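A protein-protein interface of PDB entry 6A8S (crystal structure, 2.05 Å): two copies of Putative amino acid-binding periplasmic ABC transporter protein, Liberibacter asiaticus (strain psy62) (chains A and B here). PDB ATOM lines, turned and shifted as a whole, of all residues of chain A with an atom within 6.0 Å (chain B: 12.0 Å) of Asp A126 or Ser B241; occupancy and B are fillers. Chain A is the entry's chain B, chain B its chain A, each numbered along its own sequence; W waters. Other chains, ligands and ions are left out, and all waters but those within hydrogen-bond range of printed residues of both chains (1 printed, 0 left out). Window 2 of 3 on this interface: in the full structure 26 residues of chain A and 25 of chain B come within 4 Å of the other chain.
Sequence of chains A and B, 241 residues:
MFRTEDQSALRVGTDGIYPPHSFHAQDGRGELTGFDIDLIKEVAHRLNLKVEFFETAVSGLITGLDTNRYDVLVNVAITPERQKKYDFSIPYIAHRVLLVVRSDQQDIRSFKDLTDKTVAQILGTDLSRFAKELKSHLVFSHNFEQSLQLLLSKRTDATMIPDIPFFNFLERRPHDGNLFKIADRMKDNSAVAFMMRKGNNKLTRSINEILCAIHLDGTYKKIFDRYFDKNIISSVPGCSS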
ATOM      1  N   ALA A  77      17.284  27.682 -11.094  1.00  0.00           N
ATOM      2  CA  ALA A  77      17.110  27.401  -9.675  1.00  0.00           C
ATOM      3  C   ALA A  77      17.446  25.947  -9.368  1.00  0.00           C
ATOM      4  O   ALA A  77      16.930  25.032 -10.013  1.00  0.00           O
ATOM      5  CB  ALA A  77      15.677  27.702  -9.247  1.00  0.00           C
ATOM      6  N   ILE A  78      18.275  25.742  -8.346  1.00  0.00           N
ATOM      7  CA  ILE A  78      18.706  24.409  -7.953  1.00  0.00           C
ATOM      8  C   ILE A  78      17.574  23.684  -7.250  1.00  0.00           C
ATOM      9  O   ILE A  78      16.994  24.200  -6.289  1.00  0.00           O
ATOM     10  CB  ILE A  78      19.932  24.497  -7.029  1.00  0.00           C
ATOM     11  CG1 ILE A  78      21.095  25.211  -7.715  1.00  0.00           C
ATOM     12  CG2 ILE A  78      20.324  23.124  -6.514  1.00  0.00           C
ATOM     13  CD1 ILE A  78      22.391  25.192  -6.856  1.00  0.00           C
ATOM     14  N   THR A  79      17.261  22.480  -7.721  1.00  0.00           N
ATOM     15  CA  THR A  79      16.325  21.563  -7.091  1.00  0.00           C
ATOM     16  C   THR A  79      17.001  20.212  -6.922  1.00  0.00           C
ATOM     17  O   THR A  79      17.987  19.922  -7.605  1.00  0.00           O
ATOM     18  CB  THR A  79      15.040  21.400  -7.925  1.00  0.00           C
ATOM     19  OG1 THR A  79      15.327  20.664  -9.119  1.00  0.00           O
ATOM     20  CG2 THR A  79      14.447  22.765  -8.287  1.00  0.00           C
ATOM     21  N   PRO A  80      16.515  19.369  -6.003  1.00  0.00           N
ATOM     22  CA  PRO A  80      17.149  18.049  -5.855  1.00  0.00           C
ATOM     23  C   PRO A  80      16.990  17.176  -7.084  1.00  0.00           C
ATOM     24  O   PRO A  80      17.876  16.364  -7.367  1.00  0.00           O
ATOM     25  CB  PRO A  80      16.445  17.440  -4.634  1.00  0.00           C
ATOM     26  CG  PRO A  80      15.794  18.577  -3.949  1.00  0.00           C
ATOM     27  CD  PRO A  80      15.453  19.575  -5.002  1.00  0.00           C
ATOM     28  N   ARG A  82      16.935  18.323 -10.209  1.00  0.00           N
ATOM     29  CA  ARG A  82      17.850  18.845 -11.221  1.00  0.00           C
ATOM     30  C   ARG A  82      19.306  18.501 -10.903  1.00  0.00           C
ATOM     31  O   ARG A  82      20.094  18.207 -11.814  1.00  0.00           O
ATOM     32  CB  ARG A  82      17.675  20.352 -11.360  1.00  0.00           C
ATOM     33  CG  ARG A  82      16.446  20.764 -12.158  1.00  0.00           C
ATOM     34  CD  ARG A  82      16.277  22.281 -12.194  1.00  0.00           C
ATOM     35  NE  ARG A  82      15.013  22.631 -12.841  1.00  0.00           N
ATOM     36  CZ  ARG A  82      14.411  23.805 -12.724  1.00  0.00           C
ATOM     37  NH1 ARG A  82      14.967  24.774 -11.992  1.00  0.00           N
ATOM     38  NH2 ARG A  82      13.260  24.013 -13.357  1.00  0.00           N
ATOM     39  N   ILE A 122       4.471  30.463 -15.899  1.00  0.00           N
ATOM     40  CA  ILE A 122       5.116  30.247 -17.186  1.00  0.00           C
ATOM     41  C   ILE A 122       5.057  28.763 -17.514  1.00  0.00           C
ATOM     42  O   ILE A 122       5.498  27.930 -16.718  1.00  0.00           O
ATOM     43  CB  ILE A 122       6.561  30.761 -17.166  1.00  0.00           C
ATOM     44  CG1 ILE A 122       6.578  32.302 -17.060  1.00  0.00           C
ATOM     45  CG2 ILE A 122       7.343  30.257 -18.406  1.00  0.00           C
ATOM     46  CD1 ILE A 122       7.918  32.837 -16.608  1.00  0.00           C
ATOM     47  N   GLY A 124       5.728  25.162 -18.425  1.00  0.00           N
ATOM     48  CA  GLY A 124       6.908  24.340 -18.347  1.00  0.00           C
ATOM     49  C   GLY A 124       7.754  24.515 -17.098  1.00  0.00           C
ATOM     50  O   GLY A 124       8.736  23.788 -16.951  1.00  0.00           O
ATOM     51  N   THR A 125       7.415  25.446 -16.202  1.00  0.00           N
ATOM     52  CA  THR A 125       8.264  25.735 -15.048  1.00  0.00           C
ATOM     53  C   THR A 125       7.833  24.924 -13.834  1.00  0.00           C
ATOM     54  O   THR A 125       6.703  24.440 -13.754  1.00  0.00           O
ATOM     55  CB  THR A 125       8.232  27.222 -14.686  1.00  0.00           C
ATOM     56  OG1 THR A 125       6.875  27.644 -14.484  1.00  0.00           O
ATOM     57  CG2 THR A 125       8.877  28.073 -15.773  1.00  0.00           C
ATOM     58  N   ASP A 126       8.758  24.792 -12.869  1.00  0.00           N
ATOM     59  CA  ASP A 126       8.405  24.200 -11.580  1.00  0.00           C
ATOM     60  C   ASP A 126       7.315  24.995 -10.883  1.00  0.00           C
ATOM     61  O   ASP A 126       6.499  24.415 -10.162  1.00  0.00           O
ATOM     62  CB  ASP A 126       9.625  24.101 -10.646  1.00  0.00           C
ATOM     63  CG  ASP A 126      10.650  23.061 -11.110  1.00  0.00           C
ATOM     64  OD1 ASP A 126      10.359  22.294 -12.051  1.00  0.00           O
ATOM     65  OD2 ASP A 126      11.757  23.016 -10.539  1.00  0.00           O
ATOM     66  N   LEU A 127       7.301  26.319 -11.044  1.00  0.00           N
ATOM     67  CA  LEU A 127       6.235  27.092 -10.409  1.00  0.00           C
ATOM     68  C   LEU A 127       4.882  26.769 -11.031  1.00  0.00           C
ATOM     69  O   LEU A 127       3.858  26.757 -10.330  1.00  0.00           O
ATOM     70  CB  LEU A 127       6.546  28.592 -10.487  1.00  0.00           C
ATOM     71  CG  LEU A 127       7.699  28.984  -9.541  1.00  0.00           C
ATOM     72  CD1 LEU A 127       7.995  30.494  -9.552  1.00  0.00           C
ATOM     73  CD2 LEU A 127       7.375  28.526  -8.138  1.00  0.00           C
ATOM     74  N   SER A 128       4.850  26.499 -12.335  1.00  0.00           N
ATOM     75  CA  SER A 128       3.602  26.066 -12.951  1.00  0.00           C
ATOM     76  C   SER A 128       3.182  24.709 -12.413  1.00  0.00           C
ATOM     77  O   SER A 128       1.997  24.472 -12.151  1.00  0.00           O
ATOM     78  CB  SER A 128       3.758  26.031 -14.473  1.00  0.00           C
ATOM     79  OG  SER A 128       2.560  25.629 -15.103  1.00  0.00           O
ATOM     80  N   ARG A 129       4.151  23.813 -12.216  1.00  0.00           N
ATOM     81  CA  ARG A 129       3.847  22.497 -11.670  1.00  0.00           C
ATOM     82  C   ARG A 129       3.297  22.622 -10.261  1.00  0.00           C
ATOM     83  O   ARG A 129       2.372  21.900  -9.882  1.00  0.00           O
ATOM     84  CB  ARG A 129       5.105  21.620 -11.692  1.00  0.00           C
ATOM     85  CG  ARG A 129       4.855  20.161 -11.362  1.00  0.00           C
ATOM     86  CD  ARG A 129       6.058  19.260 -11.706  1.00  0.00           C
ATOM     87  NE  ARG A 129       6.164  18.934 -13.136  1.00  0.00           N
ATOM     88  CZ  ARG A 129       5.217  18.353 -13.881  1.00  0.00           C
ATOM     89  NH1 ARG A 129       4.044  18.001 -13.361  1.00  0.00           N
ATOM     90  NH2 ARG A 129       5.450  18.113 -15.165  1.00  0.00           N
ATOM     91  N   PHE A 130       3.862  23.541  -9.474  1.00  0.00           N
ATOM     92  CA  PHE A 130       3.406  23.754  -8.109  1.00  0.00           C
ATOM     93  C   PHE A 130       1.970  24.271  -8.104  1.00  0.00           C
ATOM     94  O   PHE A 130       1.106  23.753  -7.386  1.00  0.00           O
ATOM     95  CB  PHE A 130       4.364  24.727  -7.423  1.00  0.00           C
ATOM     96  CG  PHE A 130       3.997  25.074  -6.001  1.00  0.00           C
ATOM     97  CD1 PHE A 130       3.597  24.093  -5.101  1.00  0.00           C
ATOM     98  CD2 PHE A 130       4.100  26.381  -5.552  1.00  0.00           C
ATOM     99  CE1 PHE A 130       3.271  24.413  -3.774  1.00  0.00           C
ATOM    100  CE2 PHE A 130       3.786  26.711  -4.213  1.00  0.00           C
ATOM    101  CZ  PHE A 130       3.358  25.717  -3.333  1.00  0.00           C
ATOM    102  N   ALA A 131       1.699  25.282  -8.926  1.00  0.00           N
ATOM    103  CA  ALA A 131       0.329  25.752  -9.128  1.00  0.00           C
ATOM    104  C   ALA A 131      -0.601  24.610  -9.530  1.00  0.00           C
ATOM    105  O   ALA A 131      -1.730  24.517  -9.039  1.00  0.00           O
ATOM    106  CB  ALA A 131       0.333  26.856 -10.181  1.00  0.00           C
ATOM    107  N   ARG B  46      21.586  10.083   5.162  1.00  0.00           N
ATOM    108  CA  ARG B  46      20.684  10.191   4.026  1.00  0.00           C
ATOM    109  C   ARG B  46      21.240   9.544   2.766  1.00  0.00           C
ATOM    110  O   ARG B  46      20.461   9.204   1.872  1.00  0.00           O
ATOM    111  CB  ARG B  46      20.357  11.649   3.761  1.00  0.00           C
ATOM    112  CG  ARG B  46      19.549  12.271   4.874  1.00  0.00           C
ATOM    113  CD  ARG B  46      19.061  13.642   4.498  1.00  0.00           C
ATOM    114  NE  ARG B  46      18.252  14.231   5.561  1.00  0.00           N
ATOM    115  CZ  ARG B  46      17.220  15.040   5.338  1.00  0.00           C
ATOM    116  NH1 ARG B  46      16.884  15.349   4.086  1.00  0.00           N
ATOM    117  NH2 ARG B  46      16.524  15.536   6.359  1.00  0.00           N
ATOM    118  N   ASN B 208      25.556  17.213  -2.729  1.00  0.00           N
ATOM    119  CA  ASN B 208      24.837  18.442  -3.072  1.00  0.00           C
ATOM    120  C   ASN B 208      23.338  18.225  -3.091  1.00  0.00           C
ATOM    121  O   ASN B 208      22.566  19.113  -2.704  1.00  0.00           O
ATOM    122  CB  ASN B 208      25.278  18.976  -4.432  1.00  0.00           C
ATOM    123  CG  ASN B 208      26.668  19.496  -4.410  1.00  0.00           C
ATOM    124  OD1 ASN B 208      27.270  19.627  -3.344  1.00  0.00           O
ATOM    125  ND2 ASN B 208      27.205  19.800  -5.587  1.00  0.00           N
ATOM    126  N   GLU B 209      22.902  17.070  -3.592  1.00  0.00           N
ATOM    127  CA  GLU B 209      21.476  16.801  -3.656  1.00  0.00           C
ATOM    128  C   GLU B 209      20.893  16.684  -2.262  1.00  0.00           C
ATOM    129  O   GLU B 209      19.859  17.291  -1.954  1.00  0.00           O
ATOM    130  CB  GLU B 209      21.208  15.529  -4.455  1.00  0.00           C
ATOM    131  CG  GLU B 209      19.730  15.237  -4.602  1.00  0.00           C
ATOM    132  CD  GLU B 209      19.471  13.861  -5.172  1.00  0.00           C
ATOM    133  OE1 GLU B 209      20.439  13.226  -5.657  1.00  0.00           O
ATOM    134  OE2 GLU B 209      18.303  13.417  -5.113  1.00  0.00           O
ATOM    135  N   ILE B 210      21.560  15.922  -1.396  1.00  0.00           N
ATOM    136  CA  ILE B 210      21.040  15.727  -0.049  1.00  0.00           C
ATOM    137  C   ILE B 210      21.106  17.026   0.761  1.00  0.00           C
ATOM    138  O   ILE B 210      20.237  17.285   1.610  1.00  0.00           O
ATOM    139  CB  ILE B 210      21.804  14.571   0.610  1.00  0.00           C
ATOM    140  CG1 ILE B 210      21.454  13.231  -0.056  1.00  0.00           C
ATOM    141  CG2 ILE B 210      21.608  14.543   2.111  1.00  0.00           C
ATOM    142  CD1 ILE B 210      20.023  13.065  -0.518  1.00  0.00           C
ATOM    143  N   LEU B 211      22.108  17.874   0.508  1.00  0.00           N
ATOM    144  CA  LEU B 211      22.162  19.156   1.215  1.00  0.00           C
ATOM    145  C   LEU B 211      20.996  20.050   0.806  1.00  0.00           C
ATOM    146  O   LEU B 211      20.468  20.806   1.629  1.00  0.00           O
ATOM    147  CB  LEU B 211      23.478  19.865   0.942  1.00  0.00           C
ATOM    148  CG  LEU B 211      24.718  19.419   1.704  1.00  0.00           C
ATOM    149  CD1 LEU B 211      25.917  20.089   1.066  1.00  0.00           C
ATOM    150  CD2 LEU B 211      24.580  19.807   3.159  1.00  0.00           C
ATOM    151  N   CYS B 212      20.576  19.969  -0.460  1.00  0.00           N
ATOM    152  CA  CYS B 212      19.384  20.693  -0.887  1.00  0.00           C
ATOM    153  C   CYS B 212      18.141  20.139  -0.197  1.00  0.00           C
ATOM    154  O   CYS B 212      17.287  20.900   0.276  1.00  0.00           O
ATOM    155  CB  CYS B 212      19.289  20.637  -2.416  1.00  0.00           C
ATOM    156  SG  CYS B 212      17.782  21.270  -3.174  1.00  0.00           S
ATOM    157  N   ALA B 213      18.051  18.815  -0.070  1.00  0.00           N
ATOM    158  CA  ALA B 213      16.935  18.216   0.658  1.00  0.00           C
ATOM    159  C   ALA B 213      16.980  18.557   2.145  1.00  0.00           C
ATOM    160  O   ALA B 213      15.938  18.737   2.782  1.00  0.00           O
ATOM    161  CB  ALA B 213      16.946  16.702   0.458  1.00  0.00           C
ATOM    162  N   ILE B 214      18.175  18.614   2.728  1.00  0.00           N
ATOM    163  CA  ILE B 214      18.304  19.027   4.123  1.00  0.00           C
ATOM    164  C   ILE B 214      17.817  20.464   4.300  1.00  0.00           C
ATOM    165  O   ILE B 214      17.106  20.781   5.262  1.00  0.00           O
ATOM    166  CB  ILE B 214      19.767  18.829   4.583  1.00  0.00           C
ATOM    167  CG1 ILE B 214      20.018  17.355   4.917  1.00  0.00           C
ATOM    168  CG2 ILE B 214      20.114  19.712   5.763  1.00  0.00           C
ATOM    169  CD1 ILE B 214      21.509  16.889   4.697  1.00  0.00           C
ATOM    170  N   HIS B 215      18.157  21.350   3.364  1.00  0.00           N
ATOM    171  CA  HIS B 215      17.621  22.709   3.421  1.00  0.00           C
ATOM    172  C   HIS B 215      16.099  22.694   3.375  1.00  0.00           C
ATOM    173  O   HIS B 215      15.433  23.359   4.179  1.00  0.00           O
ATOM    174  CB  HIS B 215      18.161  23.553   2.265  1.00  0.00           C
ATOM    175  CG  HIS B 215      19.474  24.211   2.540  1.00  0.00           C
ATOM    176  ND1 HIS B 215      19.578  25.464   3.107  1.00  0.00           N
ATOM    177  CD2 HIS B 215      20.745  23.797   2.306  1.00  0.00           C
ATOM    178  CE1 HIS B 215      20.854  25.790   3.218  1.00  0.00           C
ATOM    179  NE2 HIS B 215      21.582  24.796   2.738  1.00  0.00           N
ATOM    180  N   LEU B 216      15.525  21.893   2.467  1.00  0.00           N
ATOM    181  CA  LEU B 216      14.108  22.048   2.138  1.00  0.00           C
ATOM    182  C   LEU B 216      13.196  21.552   3.255  1.00  0.00           C
ATOM    183  O   LEU B 216      12.124  22.119   3.468  1.00  0.00           O
ATOM    184  CB  LEU B 216      13.783  21.332   0.817  1.00  0.00           C
ATOM    185  CG  LEU B 216      14.424  21.965  -0.413  1.00  0.00           C
ATOM    186  CD1 LEU B 216      14.459  21.008  -1.627  1.00  0.00           C
ATOM    187  CD2 LEU B 216      13.727  23.256  -0.769  1.00  0.00           C
ATOM    188  N   ASP B 217      13.593  20.525   3.995  1.00  0.00           N
ATOM    189  CA  ASP B 217      12.709  19.995   5.022  1.00  0.00           C
ATOM    190  C   ASP B 217      12.939  20.615   6.398  1.00  0.00           C
ATOM    191  O   ASP B 217      12.371  20.130   7.380  1.00  0.00           O
ATOM    192  CB  ASP B 217      12.836  18.467   5.105  1.00  0.00           C
ATOM    193  CG  ASP B 217      14.149  18.014   5.732  1.00  0.00           C
ATOM    194  OD1 ASP B 217      15.019  18.867   5.989  1.00  0.00           O
ATOM    195  OD2 ASP B 217      14.314  16.795   5.954  1.00  0.00           O
ATOM    196  N   GLY B 218      13.745  21.672   6.494  1.00  0.00           N
ATOM    197  CA  GLY B 218      14.003  22.307   7.770  1.00  0.00           C
ATOM    198  C   GLY B 218      15.169  21.746   8.560  1.00  0.00           C
ATOM    199  O   GLY B 218      15.494  22.298   9.618  1.00  0.00           O
ATOM    200  N   PRO B 237      22.158  30.453   0.671  1.00  0.00           N
ATOM    201  CA  PRO B 237      20.773  30.427   0.199  1.00  0.00           C
ATOM    202  C   PRO B 237      20.113  29.073   0.426  1.00  0.00           C
ATOM    203  O   PRO B 237      20.766  28.032   0.536  1.00  0.00           O
ATOM    204  CB  PRO B 237      20.902  30.730  -1.299  1.00  0.00           C
ATOM    205  CG  PRO B 237      22.234  31.361  -1.463  1.00  0.00           C
ATOM    206  CD  PRO B 237      23.103  30.704  -0.436  1.00  0.00           C
ATOM    207  N   GLY B 238      18.784  29.095   0.471  1.00  0.00           N
ATOM    208  CA  GLY B 238      18.018  27.872   0.518  1.00  0.00           C
ATOM    209  C   GLY B 238      18.003  27.201  -0.847  1.00  0.00           C
ATOM    210  O   GLY B 238      18.755  27.541  -1.761  1.00  0.00           O
ATOM    211  N   CYS B 239      17.122  26.219  -0.973  1.00  0.00           N
ATOM    212  CA  CYS B 239      16.987  25.449  -2.201  1.00  0.00           C
ATOM    213  C   CYS B 239      15.573  25.613  -2.758  1.00  0.00           C
ATOM    214  O   CYS B 239      14.776  26.403  -2.245  1.00  0.00           O
ATOM    215  CB  CYS B 239      17.319  23.984  -1.944  1.00  0.00           C
ATOM    216  SG  CYS B 239      18.067  23.269  -3.386  1.00  0.00           S
ATOM    217  N   SER B 240      15.262  24.867  -3.825  1.00  0.00           N
ATOM    218  CA  SER B 240      13.904  24.838  -4.368  1.00  0.00           C
ATOM    219  C   SER B 240      13.477  23.398  -4.607  1.00  0.00           C
ATOM    220  O   SER B 240      14.294  22.554  -4.986  1.00  0.00           O
ATOM    221  CB  SER B 240      13.791  25.618  -5.670  1.00  0.00           C
ATOM    222  OG  SER B 240      14.254  26.940  -5.505  1.00  0.00           O
ATOM    223  N   SER B 241      12.201  23.119  -4.376  1.00  0.00           N
ATOM    224  CA  SER B 241      11.688  21.766  -4.534  1.00  0.00           C
ATOM    225  C   SER B 241      11.454  21.466  -6.007  1.00  0.00           C
ATOM    226  O   SER B 241      10.915  22.310  -6.737  1.00  0.00           O
ATOM    227  CB  SER B 241      10.396  21.590  -3.745  1.00  0.00           C
ATOM    228  OG  SER B 241       9.349  22.349  -4.329  1.00  0.00           O
HETATM  229  O   HOH W   1      16.945  26.725  -5.443  1.00  0.00           O
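N of Ser B240 lies within hydrogen-bond range of O of Ile A78 (3.1 Å).
The side-chain sulfur (SG) of Cys B239 sits close to the backbone carbonyl oxygen (O) of Ile A78, 3.2 Å away.
N of Pro A80 lies close to SG of Cys B212 (3.6 Å).
SG of Cys B239 is disulfide-bonded to SG of Cys B212 (2.0 Å).
The side-chain hydroxyl (OG1) of Thr A79 lies within hydrogen-bond range of the backbone NH (N) of Arg A82.
The guanidinium group (NH2) of Arg A82 is in salt-bridge range of the side-chain carboxylate (OD2) of Asp A126, 3.3 Å away.
Among the printed residues, pairs that only touch across the chains: Thr A79 with Cys B212 (3.97 Å), Thr A79 with Ser B240 (3.1 Å), Thr A79 with Ser B241 (3.9 Å), Pro A80 with Glu B209 (3.5 Å), Pro A80 with Leu B216 (3.6 Å), Pro A80 with Ser B240 (3.2 Å) and Asp A126 with Ser B241 (3.96 Å).
No residue of chain B comes within 4 Å of Ala A77.
Printed residues of chain B within 4 Å of Ile A78: Cys B239 (3.2 Å) and Ser B240 (3.1 Å).
Of chain B, only Cys B212 (3.97 Å), Ser B240 (3.1 Å) and Ser B241 (3.9 Å) come within 4 Å of Thr A79.
Ile A122 touches none of the printed residues of chain B.
No residue of chain B comes within 4 Å of Gly A124.
Thr A125 touches none of the printed residues of chain B.
Of chain B, only Ser B241 (3.96 Å) comes within 4 Å of Asp A126.
No residue of chain B comes within 4 Å of Arg A129.
No residue of chain B comes within 4 Å of Phe A130.
Of the printed residues of chain A, Cys B212 touches Thr A79 and Pro A80.
Ala B213 touches none of the printed residues of chain A.
Printed residues of chain A within 4 Å of Leu B216: Pro A80.
Printed residues of chain A within 4 Å of Cys B239: Ile A78 (3.2 Å).
Printed residues of chain A within 4 Å of Ser B240: Ile A78 (3.1 Å), Thr A79 (3.1 Å) and Pro A80 (3.2 Å).
Ser B241 touches just these residues of chain A: Thr A79 (3.9 Å) and Asp A126 (3.96 Å).
Hydrophobic or aromatic side chains of chain A that line the printed part of chain B: Ile A78 and Pro A80.
Among the printed residues, no Asp or Glu carboxylate lies within 4 Å of a Lys or Arg side-chain nitrogen of the other chain.
No position is printed for both chains.
Of the 10 pairs that touch across the chains among the printed residues, none has its exchanged pair printed and touching as well.
Water W1 bridges the backbone carbonyl oxygen of Ile A78 (2.7 Å) and the side-chain hydroxyl of Ser B240 (2.7 Å).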
